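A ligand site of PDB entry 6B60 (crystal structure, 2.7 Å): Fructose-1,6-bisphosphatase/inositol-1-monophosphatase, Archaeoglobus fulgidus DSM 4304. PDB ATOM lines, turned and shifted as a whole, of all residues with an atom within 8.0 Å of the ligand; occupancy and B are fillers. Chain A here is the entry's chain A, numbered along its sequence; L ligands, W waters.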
ATOM      1  N   LEU A   7      30.274 -13.151  15.263  1.00  0.00           N
ATOM      2  CA  LEU A   7      30.680 -13.915  14.104  1.00  0.00           C
ATOM      3  C   LEU A   7      30.935 -15.390  14.418  1.00  0.00           C
ATOM      4  O   LEU A   7      30.559 -16.265  13.633  1.00  0.00           O
ATOM      5  CB  LEU A   7      31.908 -13.305  13.454  1.00  0.00           C
ATOM      6  CG  LEU A   7      32.313 -13.951  12.120  1.00  0.00           C
ATOM      7  CD1 LEU A   7      31.130 -14.064  11.167  1.00  0.00           C
ATOM      8  CD2 LEU A   7      33.469 -13.202  11.426  1.00  0.00           C
ATOM      9  N   ARG A   8      31.631 -15.680  15.517  1.00  0.00           N
ATOM     10  CA  ARG A   8      31.939 -17.070  15.881  1.00  0.00           C
ATOM     11  C   ARG A   8      30.706 -17.889  16.253  1.00  0.00           C
ATOM     12  O   ARG A   8      30.565 -19.044  15.846  1.00  0.00           O
ATOM     13  CB  ARG A   8      32.943 -17.100  17.033  1.00  0.00           C
ATOM     14  CG  ARG A   8      33.334 -18.511  17.469  1.00  0.00           C
ATOM     15  CD  ARG A   8      34.386 -18.472  18.559  1.00  0.00           C
ATOM     16  NE  ARG A   8      33.870 -17.869  19.778  1.00  0.00           N
ATOM     17  CZ  ARG A   8      33.163 -18.518  20.701  1.00  0.00           C
ATOM     18  NH1 ARG A   8      32.885 -19.806  20.523  1.00  0.00           N
ATOM     19  NH2 ARG A   8      32.727 -17.891  21.782  1.00  0.00           N
ATOM     20  N   ILE A   9      29.820 -17.267  17.023  1.00  0.00           N
ATOM     21  CA  ILE A   9      28.543 -17.821  17.440  1.00  0.00           C
ATOM     22  C   ILE A   9      27.665 -18.081  16.216  1.00  0.00           C
ATOM     23  O   ILE A   9      27.336 -19.234  15.929  1.00  0.00           O
ATOM     24  CB  ILE A   9      27.829 -16.841  18.413  1.00  0.00           C
ATOM     25  CG1 ILE A   9      28.661 -16.643  19.666  1.00  0.00           C
ATOM     26  CG2 ILE A   9      26.447 -17.333  18.808  1.00  0.00           C
ATOM     27  CD1 ILE A   9      28.405 -15.334  20.307  1.00  0.00           C
ATOM     28  N   SER A  10      27.268 -17.073  15.544  1.00  0.00           N
ATOM     29  CA  SER A  10      26.561 -17.159  14.261  1.00  0.00           C
ATOM     30  C   SER A  10      27.041 -18.319  13.381  1.00  0.00           C
ATOM     31  O   SER A  10      26.260 -19.171  12.962  1.00  0.00           O
ATOM     32  CB  SER A  10      26.741 -15.855  13.518  1.00  0.00           C
ATOM     33  OG  SER A  10      25.987 -14.834  14.144  1.00  0.00           O
ATOM     34  N   ARG A  11      28.335 -18.375  13.119  1.00  0.00           N
ATOM     35  CA  ARG A  11      28.847 -19.500  12.365  1.00  0.00           C
ATOM     36  C   ARG A  11      28.550 -20.862  13.034  1.00  0.00           C
ATOM     37  O   ARG A  11      28.106 -21.803  12.374  1.00  0.00           O
ATOM     38  CB  ARG A  11      30.319 -19.319  12.129  1.00  0.00           C
ATOM     39  CG  ARG A  11      30.523 -18.226  11.163  1.00  0.00           C
ATOM     40  CD  ARG A  11      31.947 -18.036  10.882  1.00  0.00           C
ATOM     41  NE  ARG A  11      32.098 -17.360   9.599  1.00  0.00           N
ATOM     42  CZ  ARG A  11      33.045 -16.466   9.345  1.00  0.00           C
ATOM     43  NH1 ARG A  11      33.924 -16.124  10.277  1.00  0.00           N
ATOM     44  NH2 ARG A  11      33.120 -15.907   8.158  1.00  0.00           N
ATOM     45  N   GLU A  12      28.791 -20.978  14.339  1.00  0.00           N
ATOM     46  CA  GLU A  12      28.540 -22.246  15.007  1.00  0.00           C
ATOM     47  C   GLU A  12      27.121 -22.730  14.728  1.00  0.00           C
ATOM     48  O   GLU A  12      26.889 -23.887  14.379  1.00  0.00           O
ATOM     49  CB  GLU A  12      28.739 -22.097  16.519  1.00  0.00           C
ATOM     50  CG  GLU A  12      29.730 -23.085  17.095  1.00  0.00           C
ATOM     51  CD  GLU A  12      29.449 -23.358  18.539  1.00  0.00           C
ATOM     52  OE1 GLU A  12      29.968 -22.573  19.381  1.00  0.00           O
ATOM     53  OE2 GLU A  12      28.696 -24.339  18.829  1.00  0.00           O
ATOM     54  N   ILE A  13      26.180 -21.803  14.886  1.00  0.00           N
ATOM     55  CA  ILE A  13      24.766 -22.056  14.637  1.00  0.00           C
ATOM     56  C   ILE A  13      24.428 -22.426  13.162  1.00  0.00           C
ATOM     57  O   ILE A  13      23.628 -23.294  12.868  1.00  0.00           O
ATOM     58  CB  ILE A  13      24.002 -20.798  15.025  1.00  0.00           C
ATOM     59  CG1 ILE A  13      24.183 -20.529  16.512  1.00  0.00           C
ATOM     60  CG2 ILE A  13      22.550 -20.912  14.609  1.00  0.00           C
ATOM     61  CD1 ILE A  13      23.676 -19.188  16.986  1.00  0.00           C
ATOM     62  N   ALA A  14      25.030 -21.728  12.214  1.00  0.00           N
ATOM     63  CA  ALA A  14      24.743 -22.045  10.838  1.00  0.00           C
ATOM     64  C   ALA A  14      25.142 -23.495  10.573  1.00  0.00           C
ATOM     65  O   ALA A  14      24.441 -24.219   9.838  1.00  0.00           O
ATOM     66  CB  ALA A  14      25.480 -21.109   9.922  1.00  0.00           C
ATOM     67  N   GLY A  15      26.234 -23.931  11.188  1.00  0.00           N
ATOM     68  CA  GLY A  15      26.686 -25.307  11.069  1.00  0.00           C
ATOM     69  C   GLY A  15      25.656 -26.307  11.599  1.00  0.00           C
ATOM     70  O   GLY A  15      25.226 -27.230  10.882  1.00  0.00           O
ATOM     71  N   GLU A  16      25.254 -26.113  12.850  1.00  0.00           N
ATOM     72  CA  GLU A  16      24.343 -27.046  13.519  1.00  0.00           C
ATOM     73  C   GLU A  16      22.988 -27.088  12.857  1.00  0.00           C
ATOM     74  O   GLU A  16      22.390 -28.167  12.770  1.00  0.00           O
ATOM     75  CB  GLU A  16      24.161 -26.695  15.004  1.00  0.00           C
ATOM     76  CG  GLU A  16      25.308 -27.130  15.892  1.00  0.00           C
ATOM     77  CD  GLU A  16      25.891 -28.499  15.491  1.00  0.00           C
ATOM     78  OE1 GLU A  16      25.092 -29.485  15.372  1.00  0.00           O
ATOM     79  OE2 GLU A  16      27.138 -28.582  15.298  1.00  0.00           O
ATOM     80  N   ARG A  18      22.264 -25.972   9.656  1.00  0.00           N
ATOM     81  CA  ARG A  18      22.354 -26.423   8.288  1.00  0.00           C
ATOM     82  C   ARG A  18      22.316 -27.937   8.277  1.00  0.00           C
ATOM     83  O   ARG A  18      21.645 -28.567   7.459  1.00  0.00           O
ATOM     84  CB  ARG A  18      23.639 -25.929   7.648  1.00  0.00           C
ATOM     85  CG  ARG A  18      23.821 -26.444   6.232  1.00  0.00           C
ATOM     86  CD  ARG A  18      25.298 -26.492   5.875  1.00  0.00           C
ATOM     87  NE  ARG A  18      26.015 -27.474   6.706  1.00  0.00           N
ATOM     88  CZ  ARG A  18      27.097 -27.224   7.462  1.00  0.00           C
ATOM     89  NH1 ARG A  18      27.644 -25.996   7.521  1.00  0.00           N
ATOM     90  NH2 ARG A  18      27.630 -28.211   8.170  1.00  0.00           N
ATOM     91  N   LYS A  19      23.029 -28.511   9.239  1.00  0.00           N
ATOM     92  CA  LYS A  19      23.051 -29.943   9.449  1.00  0.00           C
ATOM     93  C   LYS A  19      21.686 -30.516   9.854  1.00  0.00           C
ATOM     94  O   LYS A  19      21.224 -31.522   9.276  1.00  0.00           O
ATOM     95  CB  LYS A  19      24.124 -30.271  10.496  1.00  0.00           C
ATOM     96  CG  LYS A  19      23.984 -31.625  11.158  1.00  0.00           C
ATOM     97  CD  LYS A  19      25.371 -32.119  11.643  1.00  0.00           C
ATOM     98  CE  LYS A  19      26.171 -31.029  12.416  1.00  0.00           C
ATOM     99  NZ  LYS A  19      27.421 -31.576  13.045  1.00  0.00           N
ATOM    100  N   TYR A 116      23.719 -11.295  10.526  1.00  0.00           N
ATOM    101  CA  TYR A 116      24.173 -12.546   9.914  1.00  0.00           C
ATOM    102  C   TYR A 116      22.969 -13.234   9.280  1.00  0.00           C
ATOM    103  O   TYR A 116      21.901 -13.285   9.847  1.00  0.00           O
ATOM    104  CB  TYR A 116      24.781 -13.438  11.003  1.00  0.00           C
ATOM    105  CG  TYR A 116      25.505 -14.650  10.520  1.00  0.00           C
ATOM    106  CD1 TYR A 116      26.809 -14.566  10.038  1.00  0.00           C
ATOM    107  CD2 TYR A 116      24.928 -15.888  10.559  1.00  0.00           C
ATOM    108  CE1 TYR A 116      27.516 -15.682   9.622  1.00  0.00           C
ATOM    109  CE2 TYR A 116      25.608 -17.009  10.131  1.00  0.00           C
ATOM    110  CZ  TYR A 116      26.906 -16.905   9.656  1.00  0.00           C
ATOM    111  OH  TYR A 116      27.595 -18.020   9.237  1.00  0.00           O
ATOM    112  N   TYR A 118      22.511 -16.722   6.690  1.00  0.00           N
ATOM    113  CA  TYR A 118      23.284 -17.752   6.034  1.00  0.00           C
ATOM    114  C   TYR A 118      22.345 -18.659   5.285  1.00  0.00           C
ATOM    115  O   TYR A 118      21.489 -19.299   5.887  1.00  0.00           O
ATOM    116  CB  TYR A 118      24.067 -18.523   7.085  1.00  0.00           C
ATOM    117  CG  TYR A 118      24.737 -19.769   6.594  1.00  0.00           C
ATOM    118  CD1 TYR A 118      26.058 -19.755   6.181  1.00  0.00           C
ATOM    119  CD2 TYR A 118      24.049 -20.984   6.585  1.00  0.00           C
ATOM    120  CE1 TYR A 118      26.683 -20.925   5.745  1.00  0.00           C
ATOM    121  CE2 TYR A 118      24.665 -22.142   6.166  1.00  0.00           C
ATOM    122  CZ  TYR A 118      25.976 -22.105   5.749  1.00  0.00           C
ATOM    123  OH  TYR A 118      26.575 -23.263   5.326  1.00  0.00           O
ATOM    124  N   ASN A 119      22.478 -18.665   3.960  1.00  0.00           N
ATOM    125  CA  ASN A 119      21.609 -19.447   3.118  1.00  0.00           C
ATOM    126  C   ASN A 119      21.897 -20.916   3.322  1.00  0.00           C
ATOM    127  O   ASN A 119      23.025 -21.373   3.097  1.00  0.00           O
ATOM    128  CB  ASN A 119      21.783 -19.051   1.674  1.00  0.00           C
ATOM    129  CG  ASN A 119      20.905 -19.850   0.767  1.00  0.00           C
ATOM    130  OD1 ASN A 119      20.806 -21.067   0.901  1.00  0.00           O
ATOM    131  ND2 ASN A 119      20.260 -19.195  -0.164  1.00  0.00           N
ATOM    132  N   LEU A 120      20.870 -21.636   3.771  1.00  0.00           N
ATOM    133  CA  LEU A 120      21.046 -22.981   4.328  1.00  0.00           C
ATOM    134  C   LEU A 120      20.984 -24.018   3.232  1.00  0.00           C
ATOM    135  O   LEU A 120      21.343 -25.168   3.455  1.00  0.00           O
ATOM    136  CB  LEU A 120      19.940 -23.269   5.337  1.00  0.00           C
ATOM    137  CG  LEU A 120      20.039 -22.465   6.606  1.00  0.00           C
ATOM    138  CD1 LEU A 120      18.709 -22.448   7.368  1.00  0.00           C
ATOM    139  CD2 LEU A 120      21.111 -23.057   7.452  1.00  0.00           C
ATOM    140  N   GLY A 123      24.624 -22.488   1.202  1.00  0.00           N
ATOM    141  CA  GLY A 123      25.789 -22.126   2.011  1.00  0.00           C
ATOM    142  C   GLY A 123      26.375 -20.750   1.730  1.00  0.00           C
ATOM    143  O   GLY A 123      27.538 -20.495   2.017  1.00  0.00           O
ATOM    144  N   ASP A 124      25.598 -19.844   1.161  1.00  0.00           N
ATOM    145  CA  ASP A 124      26.024 -18.473   1.032  1.00  0.00           C
ATOM    146  C   ASP A 124      26.001 -17.823   2.409  1.00  0.00           C
ATOM    147  O   ASP A 124      25.071 -17.965   3.155  1.00  0.00           O
ATOM    148  CB  ASP A 124      25.140 -17.693   0.057  1.00  0.00           C
ATOM    149  CG  ASP A 124      25.415 -18.038  -1.388  1.00  0.00           C
ATOM    150  OD1 ASP A 124      26.593 -18.027  -1.777  1.00  0.00           O
ATOM    151  OD2 ASP A 124      24.447 -18.345  -2.114  1.00  0.00           O
ATOM    152  N   GLU A 125      27.046 -17.087   2.744  1.00  0.00           N
ATOM    153  CA  GLU A 125      27.086 -16.482   4.044  1.00  0.00           C
ATOM    154  C   GLU A 125      27.123 -14.961   3.936  1.00  0.00           C
ATOM    155  O   GLU A 125      28.086 -14.387   3.421  1.00  0.00           O
ATOM    156  CB  GLU A 125      28.292 -16.976   4.821  1.00  0.00           C
ATOM    157  CG  GLU A 125      28.401 -16.235   6.161  1.00  0.00           C
ATOM    158  CD  GLU A 125      29.739 -16.450   6.815  1.00  0.00           C
ATOM    159  OE1 GLU A 125      30.734 -15.898   6.261  1.00  0.00           O
ATOM    160  OE2 GLU A 125      29.778 -17.150   7.864  1.00  0.00           O
ATOM    161  N   ASN A 136      30.148 -14.202   1.632  1.00  0.00           N
ATOM    162  CA  ASN A 136      31.170 -15.237   1.508  1.00  0.00           C
ATOM    163  C   ASN A 136      32.560 -14.631   1.635  1.00  0.00           C
ATOM    164  O   ASN A 136      33.479 -14.970   0.882  1.00  0.00           O
ATOM    165  CB  ASN A 136      31.042 -15.997   0.194  1.00  0.00           C
ATOM    166  CG  ASN A 136      29.849 -16.914   0.149  1.00  0.00           C
ATOM    167  OD1 ASN A 136      29.672 -17.797   0.989  1.00  0.00           O
ATOM    168  ND2 ASN A 136      28.994 -16.706  -0.845  1.00  0.00           N
ATOM    169  N   GLY A 137      32.699 -13.718   2.579  1.00  0.00           N
ATOM    170  CA  GLY A 137      34.012 -13.243   2.954  1.00  0.00           C
ATOM    171  C   GLY A 137      34.441 -12.020   2.172  1.00  0.00           C
ATOM    172  O   GLY A 137      35.414 -11.390   2.539  1.00  0.00           O
HETATM  173  N1  LIG L   1      29.957 -23.065   9.934  1.00  0.00           N
HETATM  174  C1  LIG L   1      29.521 -22.252   8.749  1.00  0.00           C
HETATM  175  C2  LIG L   1      29.792 -23.051   7.474  1.00  0.00           C
HETATM  176  O1  LIG L   1      30.917 -23.169   7.006  1.00  0.00           O
HETATM  177  C3  LIG L   1      30.219 -20.874   8.730  1.00  0.00           C
HETATM  178  C4  LIG L   1      30.784 -20.363   7.390  1.00  0.00           C
HETATM  179  C5  LIG L   1      32.325 -20.503   7.297  1.00  0.00           C
HETATM  180  O2  LIG L   1      32.921 -20.081   6.289  1.00  0.00           O
HETATM  181  O3  LIG L   1      32.941 -21.046   8.250  1.00  0.00           O
HETATM  182  O4  LIG L   1      28.866 -23.617   6.870  1.00  0.00           O
HETATM  183  O   HOH W   1      34.281 -21.553   4.076  1.00  0.00           O
HETATM  184  O   HOH W   2      31.913 -22.782  12.815  1.00  0.00           O
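The backbone carbonyl oxygen of Glu 125 is in hydrogen-bond range of the backbone NH of Asn 136 (2.7 Å). The side-chain carboxylate (OE2) of Glu 125 lies within salt-bridge range of the guanidinium group (NE) of Arg 11 (2.9 Å). The side-chain carboxylate of Glu 125 lies within hydrogen-bond range of the side-chain hydroxyl of Tyr 116 (2.7 Å).
O of Arg 11 is in hydrogen-bond range of N1 of the ligand (3.3 Å). OH of Tyr 118 sits at hydrogen-bond distance from O4 of the ligand. The guanidinium group of Arg 18 is in salt-bridge range of an oxygen (O4) of the ligand, 2.8 Å away.
Merely in contact with the ligand: Glu 125 (3.4 Å) and Tyr 116 (3.9 Å). Hydrophobic or aromatic side chains that line the ligand: Tyr 118. Five residues have an atom within 4 Å of the ligand: Arg 11, Arg 18, Tyr 116, Tyr 118 and Glu 125. The nearest printed residue that does not touch the ligand is Gly 15 (4.02 Å).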
